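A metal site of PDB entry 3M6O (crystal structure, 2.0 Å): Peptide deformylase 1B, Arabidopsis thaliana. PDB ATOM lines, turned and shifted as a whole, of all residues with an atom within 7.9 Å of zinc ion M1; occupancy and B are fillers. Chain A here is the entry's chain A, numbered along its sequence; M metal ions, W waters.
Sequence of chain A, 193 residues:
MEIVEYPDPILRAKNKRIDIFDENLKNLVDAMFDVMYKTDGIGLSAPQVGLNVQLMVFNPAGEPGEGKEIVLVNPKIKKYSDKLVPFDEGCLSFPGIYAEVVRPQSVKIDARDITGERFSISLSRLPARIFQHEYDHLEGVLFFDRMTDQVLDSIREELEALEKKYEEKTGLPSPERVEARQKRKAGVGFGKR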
ATOM      1  N   ILE A   3      -8.214  11.423 -27.534  1.00  0.00           N
ATOM      2  CA  ILE A   3      -9.255  10.398 -27.280  1.00  0.00           C
ATOM      3  C   ILE A   3      -8.864   9.136 -28.007  1.00  0.00           C
ATOM      4  O   ILE A   3      -8.601   9.158 -29.212  1.00  0.00           O
ATOM      5  CB  ILE A   3     -10.736  10.856 -27.591  1.00  0.00           C
ATOM      6  CG1 ILE A   3     -11.146  11.892 -26.575  1.00  0.00           C
ATOM      7  CG2 ILE A   3     -11.823   9.688 -27.476  1.00  0.00           C
ATOM      8  CD1 ILE A   3     -11.087  13.298 -27.171  1.00  0.00           C
ATOM      9  N   VAL A   4      -8.816   8.048 -27.240  1.00  0.00           N
ATOM     10  CA  VAL A   4      -8.579   6.688 -27.721  1.00  0.00           C
ATOM     11  C   VAL A   4      -9.823   6.142 -28.357  1.00  0.00           C
ATOM     12  O   VAL A   4     -10.934   6.196 -27.770  1.00  0.00           O
ATOM     13  CB  VAL A   4      -8.144   5.733 -26.572  1.00  0.00           C
ATOM     14  CG1 VAL A   4      -7.891   4.313 -27.054  1.00  0.00           C
ATOM     15  CG2 VAL A   4      -6.956   6.286 -25.854  1.00  0.00           C
ATOM     16  N   LEU A  11      -8.785   0.405 -24.348  1.00  0.00           N
ATOM     17  CA  LEU A  11     -10.227   0.488 -24.018  1.00  0.00           C
ATOM     18  C   LEU A  11     -10.783  -0.833 -23.545  1.00  0.00           C
ATOM     19  O   LEU A  11     -11.992  -0.924 -23.206  1.00  0.00           O
ATOM     20  CB  LEU A  11     -11.065   0.936 -25.228  1.00  0.00           C
ATOM     21  CG  LEU A  11     -10.950   2.408 -25.660  1.00  0.00           C
ATOM     22  CD1 LEU A  11     -11.646   2.578 -26.971  1.00  0.00           C
ATOM     23  CD2 LEU A  11     -11.499   3.281 -24.557  1.00  0.00           C
ATOM     24  N   GLY A  43     -19.420  13.318 -18.809  1.00  0.00           N
ATOM     25  CA  GLY A  43     -18.432  12.430 -18.092  1.00  0.00           C
ATOM     26  C   GLY A  43     -17.284  12.014 -18.999  1.00  0.00           C
ATOM     27  O   GLY A  43     -17.486  11.942 -20.205  1.00  0.00           O
ATOM     28  N   LEU A  44     -16.081  11.777 -18.433  1.00  0.00           N
ATOM     29  CA  LEU A  44     -14.890  11.244 -19.128  1.00  0.00           C
ATOM     30  C   LEU A  44     -14.097  10.344 -18.208  1.00  0.00           C
ATOM     31  O   LEU A  44     -13.757  10.746 -17.071  1.00  0.00           O
ATOM     32  CB  LEU A  44     -14.002  12.360 -19.665  1.00  0.00           C
ATOM     33  CG  LEU A  44     -12.721  12.009 -20.437  1.00  0.00           C
ATOM     34  CD1 LEU A  44     -12.928  11.218 -21.724  1.00  0.00           C
ATOM     35  CD2 LEU A  44     -12.083  13.278 -20.785  1.00  0.00           C
ATOM     36  N   SER A  45     -13.822   9.115 -18.667  1.00  0.00           N
ATOM     37  CA  SER A  45     -13.065   8.111 -17.893  1.00  0.00           C
ATOM     38  C   SER A  45     -11.644   8.086 -18.424  1.00  0.00           C
ATOM     39  O   SER A  45     -11.437   8.324 -19.594  1.00  0.00           O
ATOM     40  CB  SER A  45     -13.682   6.759 -18.084  1.00  0.00           C
ATOM     41  OG  SER A  45     -13.723   6.550 -19.529  1.00  0.00           O
ATOM     42  N   GLN A  48     -10.301   6.342 -21.758  1.00  0.00           N
ATOM     43  CA  GLN A  48     -10.561   7.103 -22.981  1.00  0.00           C
ATOM     44  C   GLN A  48      -9.482   8.157 -23.312  1.00  0.00           C
ATOM     45  O   GLN A  48      -9.267   8.477 -24.476  1.00  0.00           O
ATOM     46  CB  GLN A  48     -11.966   7.688 -22.891  1.00  0.00           C
ATOM     47  CG  GLN A  48     -13.015   6.686 -23.332  1.00  0.00           C
ATOM     48  CD  GLN A  48     -14.333   7.361 -23.516  1.00  0.00           C
ATOM     49  OE1 GLN A  48     -14.839   7.948 -22.575  1.00  0.00           O
ATOM     50  NE2 GLN A  48     -14.929   7.267 -24.739  1.00  0.00           N
ATOM     51  N   GLU A  89     -27.250   6.299 -27.686  1.00  0.00           N
ATOM     52  CA  GLU A  89     -25.973   6.502 -27.067  1.00  0.00           C
ATOM     53  C   GLU A  89     -24.973   6.812 -28.146  1.00  0.00           C
ATOM     54  O   GLU A  89     -25.116   6.342 -29.276  1.00  0.00           O
ATOM     55  CB  GLU A  89     -25.544   5.288 -26.245  1.00  0.00           C
ATOM     56  CG  GLU A  89     -25.768   5.620 -24.792  1.00  0.00           C
ATOM     57  CD  GLU A  89     -25.335   4.539 -23.838  1.00  0.00           C
ATOM     58  OE1 GLU A  89     -24.112   4.225 -23.766  1.00  0.00           O
ATOM     59  OE2 GLU A  89     -26.242   4.039 -23.128  1.00  0.00           O
ATOM     60  N   GLY A  90     -24.002   7.660 -27.793  1.00  0.00           N
ATOM     61  CA  GLY A  90     -22.834   7.879 -28.618  1.00  0.00           C
ATOM     62  C   GLY A  90     -21.680   7.569 -27.748  1.00  0.00           C
ATOM     63  O   GLY A  90     -21.828   7.247 -26.572  1.00  0.00           O
ATOM     64  N   CYS A  91     -20.485   7.702 -28.312  1.00  0.00           N
ATOM     65  CA  CYS A  91     -19.319   7.371 -27.590  1.00  0.00           C
ATOM     66  C   CYS A  91     -18.187   7.976 -28.385  1.00  0.00           C
ATOM     67  O   CYS A  91     -18.052   7.705 -29.596  1.00  0.00           O
ATOM     68  CB  CYS A  91     -19.126   5.846 -27.549  1.00  0.00           C
ATOM     69  SG  CYS A  91     -17.682   5.427 -26.508  1.00  0.00           S
ATOM     70  N   LEU A  92     -17.375   8.771 -27.718  1.00  0.00           N
ATOM     71  CA  LEU A  92     -16.229   9.409 -28.354  1.00  0.00           C
ATOM     72  C   LEU A  92     -15.164   8.485 -28.973  1.00  0.00           C
ATOM     73  O   LEU A  92     -14.271   8.910 -29.778  1.00  0.00           O
ATOM     74  CB  LEU A  92     -15.561  10.345 -27.319  1.00  0.00           C
ATOM     75  CG  LEU A  92     -16.245  11.693 -26.973  1.00  0.00           C
ATOM     76  CD1 LEU A  92     -15.255  12.587 -26.365  1.00  0.00           C
ATOM     77  CD2 LEU A  92     -16.847  12.375 -28.168  1.00  0.00           C
ATOM     78  N   SER A  93     -15.172   7.235 -28.521  1.00  0.00           N
ATOM     79  CA  SER A  93     -14.243   6.243 -28.978  1.00  0.00           C
ATOM     80  C   SER A  93     -14.735   5.641 -30.233  1.00  0.00           C
ATOM     81  O   SER A  93     -14.050   4.782 -30.782  1.00  0.00           O
ATOM     82  CB  SER A  93     -13.887   5.171 -27.950  1.00  0.00           C
ATOM     83  OG  SER A  93     -13.414   5.815 -26.744  1.00  0.00           O
ATOM     84  N   PHE A  94     -15.924   6.089 -30.706  1.00  0.00           N
ATOM     85  CA  PHE A  94     -16.543   5.499 -31.959  1.00  0.00           C
ATOM     86  C   PHE A  94     -17.065   6.644 -32.704  1.00  0.00           C
ATOM     87  O   PHE A  94     -18.261   6.892 -32.576  1.00  0.00           O
ATOM     88  CB  PHE A  94     -17.752   4.589 -31.598  1.00  0.00           C
ATOM     89  CG  PHE A  94     -17.373   3.333 -30.829  1.00  0.00           C
ATOM     90  CD1 PHE A  94     -17.139   3.392 -29.460  1.00  0.00           C
ATOM     91  CD2 PHE A  94     -17.207   2.148 -31.470  1.00  0.00           C
ATOM     92  CE1 PHE A  94     -16.824   2.291 -28.755  1.00  0.00           C
ATOM     93  CE2 PHE A  94     -16.846   0.969 -30.761  1.00  0.00           C
ATOM     94  CZ  PHE A  94     -16.633   1.060 -29.379  1.00  0.00           C
ATOM     95  N   ILE A 130     -25.163   8.719 -18.670  1.00  0.00           N
ATOM     96  CA  ILE A 130     -23.802   9.002 -19.005  1.00  0.00           C
ATOM     97  C   ILE A 130     -22.872   8.318 -17.978  1.00  0.00           C
ATOM     98  O   ILE A 130     -21.850   7.779 -18.404  1.00  0.00           O
ATOM     99  CB  ILE A 130     -23.493  10.503 -19.035  1.00  0.00           C
ATOM    100  CG1 ILE A 130     -24.325  11.276 -20.097  1.00  0.00           C
ATOM    101  CG2 ILE A 130     -21.994  10.718 -19.340  1.00  0.00           C
ATOM    102  CD1 ILE A 130     -24.351  10.689 -21.543  1.00  0.00           C
ATOM    103  N   HIS A 133     -22.465   4.728 -18.880  1.00  0.00           N
ATOM    104  CA  HIS A 133     -21.589   4.671 -20.074  1.00  0.00           C
ATOM    105  C   HIS A 133     -20.086   4.732 -19.749  1.00  0.00           C
ATOM    106  O   HIS A 133     -19.302   3.919 -20.248  1.00  0.00           O
ATOM    107  CB  HIS A 133     -21.967   5.715 -21.153  1.00  0.00           C
ATOM    108  CG  HIS A 133     -21.186   5.584 -22.428  1.00  0.00           C
ATOM    109  ND1 HIS A 133     -21.736   5.088 -23.593  1.00  0.00           N
ATOM    110  CD2 HIS A 133     -19.898   5.903 -22.722  1.00  0.00           C
ATOM    111  CE1 HIS A 133     -20.828   5.120 -24.549  1.00  0.00           C
ATOM    112  NE2 HIS A 133     -19.686   5.536 -24.023  1.00  0.00           N
ATOM    113  N   GLU A 134     -19.723   5.665 -18.872  1.00  0.00           N
ATOM    114  CA  GLU A 134     -18.322   5.948 -18.570  1.00  0.00           C
ATOM    115  C   GLU A 134     -17.785   4.977 -17.511  1.00  0.00           C
ATOM    116  O   GLU A 134     -16.573   4.794 -17.346  1.00  0.00           O
ATOM    117  CB  GLU A 134     -18.188   7.383 -18.053  1.00  0.00           C
ATOM    118  CG  GLU A 134     -18.651   8.410 -19.068  1.00  0.00           C
ATOM    119  CD  GLU A 134     -17.722   8.384 -20.300  1.00  0.00           C
ATOM    120  OE1 GLU A 134     -18.210   8.397 -21.473  1.00  0.00           O
ATOM    121  OE2 GLU A 134     -16.486   8.352 -20.057  1.00  0.00           O
ATOM    122  N   ASP A 136     -18.694   1.849 -17.386  1.00  0.00           N
ATOM    123  CA  ASP A 136     -18.373   0.776 -18.290  1.00  0.00           C
ATOM    124  C   ASP A 136     -16.938   0.896 -18.837  1.00  0.00           C
ATOM    125  O   ASP A 136     -16.166  -0.026 -18.763  1.00  0.00           O
ATOM    126  CB  ASP A 136     -19.452   0.687 -19.378  1.00  0.00           C
ATOM    127  CG  ASP A 136     -20.687  -0.090 -18.918  1.00  0.00           C
ATOM    128  OD1 ASP A 136     -21.581  -0.325 -19.784  1.00  0.00           O
ATOM    129  OD2 ASP A 136     -20.755  -0.455 -17.692  1.00  0.00           O
ATOM    130  N   HIS A 137     -16.552   2.046 -19.369  1.00  0.00           N
ATOM    131  CA  HIS A 137     -15.148   2.254 -19.745  1.00  0.00           C
ATOM    132  C   HIS A 137     -14.137   1.845 -18.670  1.00  0.00           C
ATOM    133  O   HIS A 137     -13.106   1.243 -19.012  1.00  0.00           O
ATOM    134  CB  HIS A 137     -14.932   3.729 -20.139  1.00  0.00           C
ATOM    135  CG  HIS A 137     -15.489   4.077 -21.477  1.00  0.00           C
ATOM    136  ND1 HIS A 137     -15.073   3.434 -22.623  1.00  0.00           N
ATOM    137  CD2 HIS A 137     -16.443   4.977 -21.868  1.00  0.00           C
ATOM    138  CE1 HIS A 137     -15.703   3.958 -23.667  1.00  0.00           C
ATOM    139  NE2 HIS A 137     -16.522   4.911 -23.249  1.00  0.00           N
ATOM    140  N   VAL A 141     -15.557  -2.190 -20.656  1.00  0.00           N
ATOM    141  CA  VAL A 141     -16.796  -2.519 -21.378  1.00  0.00           C
ATOM    142  C   VAL A 141     -17.166  -1.335 -22.265  1.00  0.00           C
ATOM    143  O   VAL A 141     -17.081  -0.204 -21.783  1.00  0.00           O
ATOM    144  CB  VAL A 141     -17.959  -2.745 -20.387  1.00  0.00           C
ATOM    145  CG1 VAL A 141     -19.237  -3.205 -21.131  1.00  0.00           C
ATOM    146  CG2 VAL A 141     -17.554  -3.754 -19.299  1.00  0.00           C
ATOM    147  N   LEU A 142     -17.460  -1.603 -23.566  1.00  0.00           N
ATOM    148  CA  LEU A 142     -17.837  -0.639 -24.624  1.00  0.00           C
ATOM    149  C   LEU A 142     -19.293  -0.705 -24.989  1.00  0.00           C
ATOM    150  O   LEU A 142     -19.908  -1.783 -24.906  1.00  0.00           O
ATOM    151  CB  LEU A 142     -17.024  -0.899 -25.916  1.00  0.00           C
ATOM    152  CG  LEU A 142     -15.514  -0.844 -25.790  1.00  0.00           C
ATOM    153  CD1 LEU A 142     -14.883  -0.438 -27.086  1.00  0.00           C
ATOM    154  CD2 LEU A 142     -15.170   0.200 -24.785  1.00  0.00           C
ATOM    155  N   PHE A 143     -19.882   0.414 -25.434  1.00  0.00           N
ATOM    156  CA  PHE A 143     -21.375   0.453 -25.513  1.00  0.00           C
ATOM    157  C   PHE A 143     -21.976  -0.593 -26.391  1.00  0.00           C
ATOM    158  O   PHE A 143     -23.122  -1.043 -26.185  1.00  0.00           O
ATOM    159  CB  PHE A 143     -21.998   1.850 -25.783  1.00  0.00           C
ATOM    160  CG  PHE A 143     -21.830   2.379 -27.188  1.00  0.00           C
ATOM    161  CD1 PHE A 143     -22.723   3.303 -27.693  1.00  0.00           C
ATOM    162  CD2 PHE A 143     -20.731   2.017 -27.997  1.00  0.00           C
ATOM    163  CE1 PHE A 143     -22.567   3.834 -28.980  1.00  0.00           C
ATOM    164  CE2 PHE A 143     -20.595   2.512 -29.258  1.00  0.00           C
ATOM    165  CZ  PHE A 143     -21.483   3.446 -29.736  1.00  0.00           C
HETATM  166 ZN    ZN M   1     -17.658   6.081 -24.499  1.00  0.00          ZN
HETATM  167 ZN    ZN M   2     -16.552   8.939 -22.672  1.00  0.00          ZN
HETATM  168  O   HOH W   1     -17.248   7.959 -24.019  1.00  0.00           O
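Gln 48 touches zinc ion M1. Glu 134 touches zinc ion M1. Of the 21 residues printed, 5 come within 4 Å of zinc ion M1. The nearest printed residue that does not touch zinc ion M1 is Leu 92 (4.2 Å).
The side-chain amide nitrogen (NE2) of Gln 48 lies close to a ring nitrogen (NE2) of His 137 (3.2 Å). The side-chain amide nitrogen (NE2) of Gln 48 sits close to the side-chain sulfur (SG) of Cys 91 (3.8 Å). SG of Cys 91 sits close to N of Ser 93, 3.7 Å away. OE1 of Glu 89 is in hydrogen-bond range of ND1 of His 133. The side-chain amide nitrogen (NE2) of Gln 48 is in hydrogen-bond range of the side-chain hydroxyl (OG) of Ser 93 (2.9 Å). The backbone carbonyl oxygen (O) of Gln 48 is in hydrogen-bond range of the backbone NH (N) of Val 4, 2.8 Å away. OE2 of Glu 134 is in hydrogen-bond range of N of Ser 45 (3.1 Å).
Zinc ion M1 is bound by water W1 (2.0 Å), NE2 of His 137 (2.1 Å), SG of Cys 91 (2.1 Å) and NE2 of His 133 (2.2 Å). Zinc ion M1 has four donor atoms within binding distance.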
